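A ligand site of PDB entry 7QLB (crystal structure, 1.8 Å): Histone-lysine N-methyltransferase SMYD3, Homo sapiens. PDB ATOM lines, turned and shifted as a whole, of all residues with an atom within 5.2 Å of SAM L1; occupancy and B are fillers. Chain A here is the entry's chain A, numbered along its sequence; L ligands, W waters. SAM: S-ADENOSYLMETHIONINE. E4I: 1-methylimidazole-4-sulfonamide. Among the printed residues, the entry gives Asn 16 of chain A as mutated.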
ATOM      1  N   ASN A  16      -7.938  -1.012  15.304  1.00  0.00           N
ATOM      2  CA  ASN A  16      -7.770  -0.495  13.950  1.00  0.00           C
ATOM      3  C   ASN A  16      -6.781  -1.261  13.085  1.00  0.00           C
ATOM      4  O   ASN A  16      -6.302  -0.704  12.081  1.00  0.00           O
ATOM      5  CB  ASN A  16      -7.339   0.996  13.979  1.00  0.00           C
ATOM      6  CG  ASN A  16      -6.056   1.223  14.757  1.00  0.00           C
ATOM      7  OD1 ASN A  16      -5.086   0.485  14.625  1.00  0.00           O
ATOM      8  ND2 ASN A  16      -6.041   2.268  15.572  1.00  0.00           N
ATOM      9  N   ARG A  17      -6.441  -2.496  13.417  1.00  0.00           N
ATOM     10  CA  ARG A  17      -5.606  -3.306  12.541  1.00  0.00           C
ATOM     11  C   ARG A  17      -6.164  -4.708  12.396  1.00  0.00           C
ATOM     12  O   ARG A  17      -5.416  -5.677  12.272  1.00  0.00           O
ATOM     13  CB  ARG A  17      -4.151  -3.328  13.006  1.00  0.00           C
ATOM     14  CG  ARG A  17      -3.932  -3.000  14.466  1.00  0.00           C
ATOM     15  CD  ARG A  17      -2.559  -2.371  14.669  1.00  0.00           C
ATOM     16  NE  ARG A  17      -1.835  -2.970  15.770  1.00  0.00           N
ATOM     17  CZ  ARG A  17      -0.769  -2.449  16.351  1.00  0.00           C
ATOM     18  NH1 ARG A  17      -0.175  -3.037  17.372  1.00  0.00           N
ATOM     19  NH2 ARG A  17      -0.304  -1.286  15.906  1.00  0.00           N
ATOM     20  N   GLY A  18      -7.482  -4.834  12.402  1.00  0.00           N
ATOM     21  CA  GLY A  18      -8.085  -6.138  12.190  1.00  0.00           C
ATOM     22  C   GLY A  18      -7.932  -7.033  13.403  1.00  0.00           C
ATOM     23  O   GLY A  18      -7.887  -6.591  14.544  1.00  0.00           O
ATOM     24  N   ASN A  19      -7.864  -8.331  13.141  1.00  0.00           N
ATOM     25  CA  ASN A  19      -7.590  -9.298  14.199  1.00  0.00           C
ATOM     26  C   ASN A  19      -6.118  -9.269  14.585  1.00  0.00           C
ATOM     27  O   ASN A  19      -5.239  -8.904  13.784  1.00  0.00           O
ATOM     28  CB  ASN A  19      -7.997 -10.706  13.754  1.00  0.00           C
ATOM     29  CG  ASN A  19      -9.476 -10.826  13.551  1.00  0.00           C
ATOM     30  OD1 ASN A  19     -10.255 -10.365  14.379  1.00  0.00           O
ATOM     31  ND2 ASN A  19      -9.883 -11.450  12.451  1.00  0.00           N
ATOM     32  N   GLY A  20      -5.854  -9.671  15.831  1.00  0.00           N
ATOM     33  CA  GLY A  20      -4.502  -9.742  16.346  1.00  0.00           C
ATOM     34  C   GLY A  20      -4.372 -10.838  17.374  1.00  0.00           C
ATOM     35  O   GLY A  20      -5.310 -11.612  17.614  1.00  0.00           O
ATOM     36  N   TYR A 127      -6.584 -19.768  13.746  1.00  0.00           N
ATOM     37  CA  TYR A 127      -6.909 -18.932  12.603  1.00  0.00           C
ATOM     38  C   TYR A 127      -6.654 -19.801  11.382  1.00  0.00           C
ATOM     39  O   TYR A 127      -5.610 -20.462  11.307  1.00  0.00           O
ATOM     40  CB  TYR A 127      -6.046 -17.683  12.592  1.00  0.00           C
ATOM     41  CG  TYR A 127      -6.622 -16.394  11.996  1.00  0.00           C
ATOM     42  CD1 TYR A 127      -7.830 -15.882  12.437  1.00  0.00           C
ATOM     43  CD2 TYR A 127      -5.893 -15.647  11.073  1.00  0.00           C
ATOM     44  CE1 TYR A 127      -8.318 -14.695  11.935  1.00  0.00           C
ATOM     45  CE2 TYR A 127      -6.366 -14.419  10.585  1.00  0.00           C
ATOM     46  CZ  TYR A 127      -7.589 -13.969  11.024  1.00  0.00           C
ATOM     47  OH  TYR A 127      -8.063 -12.768  10.571  1.00  0.00           O
ATOM     48  N   ASP A 131      -9.994 -17.681   7.193  1.00  0.00           N
ATOM     49  CA  ASP A 131     -10.085 -16.467   7.989  1.00  0.00           C
ATOM     50  C   ASP A 131      -9.119 -15.373   7.551  1.00  0.00           C
ATOM     51  O   ASP A 131      -9.272 -14.226   7.982  1.00  0.00           O
ATOM     52  CB  ASP A 131      -9.751 -16.760   9.463  1.00  0.00           C
ATOM     53  CG  ASP A 131     -10.698 -17.731  10.122  1.00  0.00           C
ATOM     54  OD1 ASP A 131     -11.928 -17.653   9.859  1.00  0.00           O
ATOM     55  OD2 ASP A 131     -10.202 -18.530  10.943  1.00  0.00           O
ATOM     56  N   LEU A 132      -8.116 -15.697   6.757  1.00  0.00           N
ATOM     57  CA  LEU A 132      -7.016 -14.770   6.521  1.00  0.00           C
ATOM     58  C   LEU A 132      -7.485 -13.478   5.868  1.00  0.00           C
ATOM     59  O   LEU A 132      -8.430 -13.441   5.072  1.00  0.00           O
ATOM     60  CB  LEU A 132      -5.951 -15.411   5.636  1.00  0.00           C
ATOM     61  CG  LEU A 132      -5.211 -16.622   6.218  1.00  0.00           C
ATOM     62  CD1 LEU A 132      -4.277 -17.205   5.159  1.00  0.00           C
ATOM     63  CD2 LEU A 132      -4.412 -16.248   7.481  1.00  0.00           C
ATOM     64  N   GLU A 133      -6.782 -12.401   6.224  1.00  0.00           N
ATOM     65  CA  GLU A 133      -7.013 -11.100   5.623  1.00  0.00           C
ATOM     66  C   GLU A 133      -6.619 -11.102   4.151  1.00  0.00           C
ATOM     67  O   GLU A 133      -5.534 -11.590   3.792  1.00  0.00           O
ATOM     68  CB  GLU A 133      -6.199 -10.050   6.357  1.00  0.00           C
ATOM     69  CG  GLU A 133      -6.279  -8.669   5.722  1.00  0.00           C
ATOM     70  CD  GLU A 133      -7.622  -8.056   5.950  1.00  0.00           C
ATOM     71  OE1 GLU A 133      -7.894  -7.684   7.124  1.00  0.00           O
ATOM     72  OE2 GLU A 133      -8.391  -7.975   4.972  1.00  0.00           O
ATOM     73  N   ASN A 135      -7.355  -7.980   2.225  1.00  0.00           N
ATOM     74  CA  ASN A 135      -7.223  -6.571   1.877  1.00  0.00           C
ATOM     75  C   ASN A 135      -7.809  -6.223   0.512  1.00  0.00           C
ATOM     76  O   ASN A 135      -7.378  -5.260  -0.139  1.00  0.00           O
ATOM     77  CB  ASN A 135      -5.773  -6.132   1.958  1.00  0.00           C
ATOM     78  CG  ASN A 135      -5.296  -5.983   3.371  1.00  0.00           C
ATOM     79  OD1 ASN A 135      -5.948  -5.330   4.181  1.00  0.00           O
ATOM     80  ND2 ASN A 135      -4.188  -6.576   3.678  1.00  0.00           N
ATOM     81  N   CYS A 183      -0.345 -11.167   1.380  1.00  0.00           N
ATOM     82  CA  CYS A 183      -0.104 -10.495   2.643  1.00  0.00           C
ATOM     83  C   CYS A 183      -0.019 -11.446   3.821  1.00  0.00           C
ATOM     84  O   CYS A 183       0.013 -10.999   4.971  1.00  0.00           O
ATOM     85  CB  CYS A 183      -1.175  -9.435   2.902  1.00  0.00           C
ATOM     86  SG  CYS A 183      -2.831 -10.048   3.019  1.00  0.00           S
ATOM     87  N   ASN A 184       0.082 -12.767   3.576  1.00  0.00           N
ATOM     88  CA  ASN A 184       0.250 -13.731   4.667  1.00  0.00           C
ATOM     89  C   ASN A 184       1.325 -14.764   4.389  1.00  0.00           C
ATOM     90  O   ASN A 184       1.441 -15.752   5.144  1.00  0.00           O
ATOM     91  CB  ASN A 184      -1.075 -14.437   4.948  1.00  0.00           C
ATOM     92  CG  ASN A 184      -2.132 -13.485   5.481  1.00  0.00           C
ATOM     93  OD1 ASN A 184      -2.074 -13.067   6.654  1.00  0.00           O
ATOM     94  ND2 ASN A 184      -3.085 -13.119   4.617  1.00  0.00           N
ATOM     95  N   SER A 205      -0.249 -15.994  11.279  1.00  0.00           N
ATOM     96  CA  SER A 205      -0.657 -14.812  10.531  1.00  0.00           C
ATOM     97  C   SER A 205      -1.544 -13.872  11.347  1.00  0.00           C
ATOM     98  O   SER A 205      -1.833 -12.769  10.881  1.00  0.00           O
ATOM     99  CB  SER A 205      -1.404 -15.224   9.258  1.00  0.00           C
ATOM    100  OG  SER A 205      -0.500 -15.662   8.270  1.00  0.00           O
ATOM    101  N   LEU A 206      -1.989 -14.275  12.534  1.00  0.00           N
ATOM    102  CA  LEU A 206      -2.721 -13.354  13.396  1.00  0.00           C
ATOM    103  C   LEU A 206      -1.837 -12.211  13.887  1.00  0.00           C
ATOM    104  O   LEU A 206      -2.340 -11.145  14.245  1.00  0.00           O
ATOM    105  CB  LEU A 206      -3.294 -14.087  14.599  1.00  0.00           C
ATOM    106  CG  LEU A 206      -4.696 -14.668  14.461  1.00  0.00           C
ATOM    107  CD1 LEU A 206      -5.068 -15.531  15.695  1.00  0.00           C
ATOM    108  CD2 LEU A 206      -5.670 -13.532  14.290  1.00  0.00           C
ATOM    109  N   LEU A 207      -0.521 -12.405  13.949  1.00  0.00           N
ATOM    110  CA  LEU A 207       0.356 -11.382  14.511  1.00  0.00           C
ATOM    111  C   LEU A 207       0.433 -10.169  13.591  1.00  0.00           C
ATOM    112  O   LEU A 207       0.782 -10.291  12.415  1.00  0.00           O
ATOM    113  CB  LEU A 207       1.753 -11.949  14.773  1.00  0.00           C
ATOM    114  CG  LEU A 207       1.847 -13.032  15.861  1.00  0.00           C
ATOM    115  CD1 LEU A 207       2.899 -14.072  15.459  1.00  0.00           C
ATOM    116  CD2 LEU A 207       2.199 -12.403  17.178  1.00  0.00           C
ATOM    117  N   ASN A 208       0.131  -8.989  14.140  1.00  0.00           N
ATOM    118  CA  ASN A 208       0.360  -7.751  13.419  1.00  0.00           C
ATOM    119  C   ASN A 208       1.821  -7.301  13.504  1.00  0.00           C
ATOM    120  O   ASN A 208       2.626  -7.828  14.277  1.00  0.00           O
ATOM    121  CB  ASN A 208      -0.587  -6.697  13.965  1.00  0.00           C
ATOM    122  CG  ASN A 208      -2.020  -6.961  13.512  1.00  0.00           C
ATOM    123  OD1 ASN A 208      -2.256  -7.211  12.327  1.00  0.00           O
ATOM    124  ND2 ASN A 208      -2.972  -6.917  14.430  1.00  0.00           N
ATOM    125  N   HIS A 209       2.145  -6.308  12.686  1.00  0.00           N
ATOM    126  CA  HIS A 209       3.513  -5.852  12.489  1.00  0.00           C
ATOM    127  C   HIS A 209       3.888  -4.726  13.428  1.00  0.00           C
ATOM    128  O   HIS A 209       3.073  -3.874  13.776  1.00  0.00           O
ATOM    129  CB  HIS A 209       3.683  -5.347  11.052  1.00  0.00           C
ATOM    130  CG  HIS A 209       4.901  -4.503  10.857  1.00  0.00           C
ATOM    131  ND1 HIS A 209       6.141  -5.032  10.556  1.00  0.00           N
ATOM    132  CD2 HIS A 209       5.083  -3.152  10.952  1.00  0.00           C
ATOM    133  CE1 HIS A 209       7.011  -4.049  10.430  1.00  0.00           C
ATOM    134  NE2 HIS A 209       6.411  -2.901  10.703  1.00  0.00           N
ATOM    135  N   SER A 210       5.163  -4.708  13.817  1.00  0.00           N
ATOM    136  CA  SER A 210       5.786  -3.529  14.425  1.00  0.00           C
ATOM    137  C   SER A 210       7.225  -3.403  13.941  1.00  0.00           C
ATOM    138  O   SER A 210       7.900  -4.414  13.731  1.00  0.00           O
ATOM    139  CB  SER A 210       5.792  -3.631  15.953  1.00  0.00           C
ATOM    140  OG  SER A 210       6.463  -2.500  16.480  1.00  0.00           O
ATOM    141  N   TYR A 242       7.604  -7.620  10.210  1.00  0.00           N
ATOM    142  CA  TYR A 242       7.472  -8.338   8.955  1.00  0.00           C
ATOM    143  C   TYR A 242       8.695  -8.178   8.055  1.00  0.00           C
ATOM    144  O   TYR A 242       8.824  -8.919   7.078  1.00  0.00           O
ATOM    145  CB  TYR A 242       6.249  -7.847   8.158  1.00  0.00           C
ATOM    146  CG  TYR A 242       4.871  -8.103   8.753  1.00  0.00           C
ATOM    147  CD1 TYR A 242       4.702  -8.813   9.930  1.00  0.00           C
ATOM    148  CD2 TYR A 242       3.732  -7.621   8.110  1.00  0.00           C
ATOM    149  CE1 TYR A 242       3.416  -9.018  10.453  1.00  0.00           C
ATOM    150  CE2 TYR A 242       2.475  -7.835   8.616  1.00  0.00           C
ATOM    151  CZ  TYR A 242       2.311  -8.547   9.780  1.00  0.00           C
ATOM    152  OH  TYR A 242       1.010  -8.749  10.266  1.00  0.00           O
ATOM    153  N   TYR A 260       1.250  -5.202   2.134  1.00  0.00           N
ATOM    154  CA  TYR A 260       0.333  -5.408   3.250  1.00  0.00           C
ATOM    155  C   TYR A 260      -0.777  -4.366   3.364  1.00  0.00           C
ATOM    156  O   TYR A 260      -1.610  -4.466   4.287  1.00  0.00           O
ATOM    157  CB  TYR A 260       1.108  -5.429   4.562  1.00  0.00           C
ATOM    158  CG  TYR A 260       2.143  -6.558   4.634  1.00  0.00           C
ATOM    159  CD1 TYR A 260       1.754  -7.861   4.909  1.00  0.00           C
ATOM    160  CD2 TYR A 260       3.479  -6.309   4.389  1.00  0.00           C
ATOM    161  CE1 TYR A 260       2.658  -8.887   4.978  1.00  0.00           C
ATOM    162  CE2 TYR A 260       4.421  -7.368   4.456  1.00  0.00           C
ATOM    163  CZ  TYR A 260       3.989  -8.636   4.745  1.00  0.00           C
ATOM    164  OH  TYR A 260       4.895  -9.664   4.784  1.00  0.00           O
ATOM    165  N   CYS A 261      -0.803  -3.387   2.486  1.00  0.00           N
ATOM    166  CA  CYS A 261      -1.857  -2.375   2.465  1.00  0.00           C
ATOM    167  C   CYS A 261      -2.106  -1.714   3.824  1.00  0.00           C
ATOM    168  O   CYS A 261      -3.260  -1.571   4.259  1.00  0.00           O
ATOM    169  CB  CYS A 261      -3.180  -2.954   1.940  1.00  0.00           C
ATOM    170  SG  CYS A 261      -3.141  -3.522   0.234  1.00  0.00           S
ATOM    171  N   PHE A 262      -1.042  -1.269   4.488  1.00  0.00           N
ATOM    172  CA  PHE A 262      -1.284  -0.370   5.623  1.00  0.00           C
ATOM    173  C   PHE A 262      -0.164   0.651   5.761  1.00  0.00           C
ATOM    174  O   PHE A 262       0.932   0.496   5.202  1.00  0.00           O
ATOM    175  CB  PHE A 262      -1.493  -1.164   6.937  1.00  0.00           C
ATOM    176  CG  PHE A 262      -0.220  -1.746   7.530  1.00  0.00           C
ATOM    177  CD1 PHE A 262       0.200  -3.003   7.145  1.00  0.00           C
ATOM    178  CD2 PHE A 262       0.508  -1.052   8.467  1.00  0.00           C
ATOM    179  CE1 PHE A 262       1.359  -3.541   7.666  1.00  0.00           C
ATOM    180  CE2 PHE A 262       1.658  -1.580   8.990  1.00  0.00           C
ATOM    181  CZ  PHE A 262       2.090  -2.818   8.615  1.00  0.00           C
ATOM    182  N   GLU A 263      -0.495   1.717   6.504  1.00  0.00           N
ATOM    183  CA  GLU A 263       0.415   2.815   6.842  1.00  0.00           C
ATOM    184  C   GLU A 263       0.853   2.617   8.290  1.00  0.00           C
ATOM    185  O   GLU A 263       0.000   2.447   9.170  1.00  0.00           O
ATOM    186  CB  GLU A 263      -0.280   4.160   6.699  1.00  0.00           C
ATOM    187  CG  GLU A 263      -1.204   4.339   5.476  1.00  0.00           C
ATOM    188  CD  GLU A 263      -0.472   4.234   4.148  1.00  0.00           C
ATOM    189  OE1 GLU A 263       0.784   4.341   4.141  1.00  0.00           O
ATOM    190  OE2 GLU A 263      -1.145   4.071   3.120  1.00  0.00           O
ATOM    191  N   CYS A 264       2.139   2.670   8.554  1.00  0.00           N
ATOM    192  CA  CYS A 264       2.647   2.380   9.900  1.00  0.00           C
ATOM    193  C   CYS A 264       2.776   3.664  10.700  1.00  0.00           C
ATOM    194  O   CYS A 264       3.436   4.617  10.257  1.00  0.00           O
ATOM    195  CB  CYS A 264       3.991   1.673   9.860  1.00  0.00           C
ATOM    196  SG  CYS A 264       4.458   1.164  11.583  1.00  0.00           S
ATOM    197  N   ASP A 265       2.172   3.660  11.890  1.00  0.00           N
ATOM    198  CA  ASP A 265       2.083   4.797  12.786  1.00  0.00           C
ATOM    199  C   ASP A 265       3.072   4.730  13.955  1.00  0.00           C
ATOM    200  O   ASP A 265       2.996   5.577  14.852  1.00  0.00           O
ATOM    201  CB  ASP A 265       0.643   4.918  13.359  1.00  0.00           C
ATOM    202  CG  ASP A 265       0.213   3.706  14.185  1.00  0.00           C
ATOM    203  OD1 ASP A 265       0.880   2.638  14.129  1.00  0.00           O
ATOM    204  OD2 ASP A 265      -0.843   3.783  14.882  1.00  0.00           O
HETATM  205  N   SAM L   1      -4.741  -8.113  11.100  1.00  0.00           N
HETATM  206  CA  SAM L   1      -4.557  -9.337  10.345  1.00  0.00           C
HETATM  207  C   SAM L   1      -5.885 -10.075  10.273  1.00  0.00           C
HETATM  208  O   SAM L   1      -5.920 -11.209   9.768  1.00  0.00           O
HETATM  209  OXT SAM L   1      -6.905  -9.550  10.708  1.00  0.00           O
HETATM  210  CB  SAM L   1      -3.461 -10.166  11.006  1.00  0.00           C
HETATM  211  CG  SAM L   1      -2.054  -9.994  10.376  1.00  0.00           C
HETATM  212  SD  SAM L   1      -1.950 -10.278   8.688  1.00  0.00           S
HETATM  213  CE  SAM L   1      -0.577 -11.329   8.540  1.00  0.00           C
HETATM  214  C5' SAM L   1      -1.403  -8.836   7.958  1.00  0.00           C
HETATM  215  C4' SAM L   1      -2.436  -7.697   7.793  1.00  0.00           C
HETATM  216  O4' SAM L   1      -2.713  -7.225   9.033  1.00  0.00           O
HETATM  217  C3' SAM L   1      -1.857  -6.512   6.973  1.00  0.00           C
HETATM  218  O3' SAM L   1      -2.031  -6.626   5.635  1.00  0.00           O
HETATM  219  C2' SAM L   1      -2.693  -5.360   7.604  1.00  0.00           C
HETATM  220  O2' SAM L   1      -4.066  -5.411   7.045  1.00  0.00           O
HETATM  221  C1' SAM L   1      -2.797  -5.662   8.917  1.00  0.00           C
HETATM  222  N9  SAM L   1      -1.803  -4.990   9.737  1.00  0.00           N
HETATM  223  C8  SAM L   1      -0.803  -5.791  10.135  1.00  0.00           C
HETATM  224  N7  SAM L   1       0.047  -5.073  10.924  1.00  0.00           N
HETATM  225  C5  SAM L   1      -0.516  -3.783  11.002  1.00  0.00           C
HETATM  226  C6  SAM L   1      -0.131  -2.617  11.627  1.00  0.00           C
HETATM  227  N6  SAM L   1       0.927  -2.169  12.450  1.00  0.00           N
HETATM  228  N1  SAM L   1      -0.873  -1.515  11.498  1.00  0.00           N
HETATM  229  C2  SAM L   1      -2.010  -1.516  10.775  1.00  0.00           C
HETATM  230  N3  SAM L   1      -2.427  -2.652  10.139  1.00  0.00           N
HETATM  231  C4  SAM L   1      -1.632  -3.767  10.293  1.00  0.00           C
HETATM  232  C1  E4I L   2       3.680 -12.342   6.569  1.00  0.00           C
HETATM  233  C2  E4I L   2       5.290 -12.379   8.027  1.00  0.00           C
HETATM  234  C3  E4I L   2       4.147 -12.737   8.669  1.00  0.00           C
HETATM  235  N   E4I L   2       3.138 -12.755   7.739  1.00  0.00           N
HETATM  236  C   E4I L   2       1.780 -13.264   7.957  1.00  0.00           C
HETATM  237  O   E4I L   2       7.601 -11.625   7.534  1.00  0.00           O
HETATM  238  N1  E4I L   2       4.967 -12.099   6.669  1.00  0.00           N
HETATM  239  N2  E4I L   2       6.927 -11.514   9.880  1.00  0.00           N
HETATM  240  O1  E4I L   2       7.262 -13.700   8.848  1.00  0.00           O
HETATM  241  S   E4I L   2       6.901 -12.340   8.533  1.00  0.00           S
HETATM  242  C1  E4I L   3     -10.410  -6.368   8.406  1.00  0.00           C
HETATM  243  C2  E4I L   3     -10.049  -4.815   6.948  1.00  0.00           C
HETATM  244  C3  E4I L   3     -10.725  -4.247   7.980  1.00  0.00           C
HETATM  245  N   E4I L   3     -10.940  -5.236   8.905  1.00  0.00           N
HETATM  246  C   E4I L   3     -11.604  -5.071  10.197  1.00  0.00           C
HETATM  247  O   E4I L   3      -8.011  -4.175   5.713  1.00  0.00           O
HETATM  248  N1  E4I L   3      -9.857  -6.172   7.238  1.00  0.00           N
HETATM  249  N2  E4I L   3      -9.758  -5.311   4.428  1.00  0.00           N
HETATM  250  O1  E4I L   3     -10.162  -3.037   5.221  1.00  0.00           O
HETATM  251  S   E4I L   3      -9.423  -4.225   5.527  1.00  0.00           S
HETATM  252  O   HOH W   1      -9.082  -9.550   9.108  1.00  0.00           O
HETATM  253  O   HOH W   2      -6.080  -6.727   9.013  1.00  0.00           O
HETATM  254  O   HOH W   3      -4.789  -3.166   5.765  1.00  0.00           O
HETATM  255  O   HOH W   4       1.994   0.241  13.424  1.00  0.00           O
HETATM  256  O   HOH W   5      -4.594 -12.709   7.896  1.00  0.00           O
HETATM  257  O   HOH W   6      -4.004   1.170  11.679  1.00  0.00           O
HETATM  258  O   HOH W   7      -4.849  -2.194   8.637  1.00  0.00           O
HETATM  259  O   HOH W   8      -0.549   1.391  11.862  1.00  0.00           O
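The side-chain amide oxygen (OD1) of Asn 184 sits close to a sulfur (SD) of SAM L1. O of Ser 205 lies close to SD of SAM L1, at 3.3 Å. The side-chain hydroxyl (OH) of Tyr 242 sits close to a sulfur (SD) of SAM L1 (3.7 Å). Gly 18 touches SAM L1 (C to OXT, 3.8 Å). CB of Glu 133 touches O of SAM L1 (3.6 Å). Cys 183 touches SAM L1. Leu 206 touches SAM L1 (O to CB, 3.6 Å). O of Leu 207 touches CG of SAM L1 (3.5 Å). Phe 262 touches SAM L1 (CE2 to C6, 3.4 Å). Hydrophobic or aromatic side chains that line SAM L1: Tyr 127, His 209, Tyr 260 and Phe 262. The nearest printed residue that does not touch SAM L1 is Asn 16 (4.6 Å).
Water W1 bridges an oxygen (OXT) of SAM L1 (2.7 Å) and the side-chain carboxylate (OE1) of Glu 133 (3.0 Å). Water W5 lies within hydrogen-bond range of an oxygen (O) of SAM L1 (2.7 Å), the backbone NH (N) of Glu 133 (2.8 Å) and the side-chain amide oxygen (OD1) of Asn 184 (2.8 Å). Water W4 lies within hydrogen-bond range of the side-chain carboxylate of Asp 265 and a nitrogen (N6) of SAM L1. Water W2 lies within hydrogen-bond range of OE1 of Glu 133 (2.8 Å), N of SAM L1 (2.8 Å) and O of Arg 17 (3.5 Å).
OD1 of Asn 184 sits at hydrogen-bond distance from OG of Ser 205 (3.4 Å). The backbone NH (N) of Asn 135 sits at hydrogen-bond distance from the side-chain carboxylate (OE2) of Glu 133 (2.9 Å). OH of Tyr 127 sits at hydrogen-bond distance from O of Asp 131 (3.2 Å). The side-chain amide nitrogen (ND2) of Asn 135 is in hydrogen-bond range of the side-chain sulfur (SG) of Cys 183, at 3.8 Å. OH of Tyr 242 sits at hydrogen-bond distance from O of Leu 207 (2.7 Å). SG of Cys 183 lies within hydrogen-bond range of ND2 of Asn 184, at 3.5 Å. O of Arg 17 sits at hydrogen-bond distance from ND2 of Asn 208 (3.5 Å). O of Tyr 260 is in hydrogen-bond range of ND2 of Asn 135, 3.4 Å away.
A nitrogen (N1) of E4I L3 sits at hydrogen-bond distance from the side-chain carboxylate of Glu 133 (2.5 Å). O of E4I L3 sits close to OD1 of Asn 135 (2.8 Å). O3' of SAM L1 is in hydrogen-bond range of ND2 of Asn 135 (2.9 Å). O of Arg 17 is in hydrogen-bond range of N of SAM L1 (2.8 Å). N of SAM L1 is in hydrogen-bond range of O of Asn 19 (2.8 Å). The side-chain amide oxygen (OD1) of Asn 208 sits at hydrogen-bond distance from a nitrogen (N) of SAM L1, at 2.9 Å. N of His 209 sits at hydrogen-bond distance from N7 of SAM L1 (3.0 Å). The backbone carbonyl oxygen of Tyr 260 is in hydrogen-bond range of an oxygen (O3') of SAM L1 (2.6 Å). The backbone NH (N) of Asn 19 sits at hydrogen-bond distance from an oxygen (OXT) of SAM L1 (2.9 Å). The side-chain hydroxyl (OH) of Tyr 127 is in hydrogen-bond range of an oxygen (O) of SAM L1. N1 of E4I L2 lies within hydrogen-bond range of OH of Tyr 260 (3.1 Å). The backbone carbonyl oxygen of His 209 sits at hydrogen-bond distance from a nitrogen (N6) of SAM L1 (3.0 Å).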
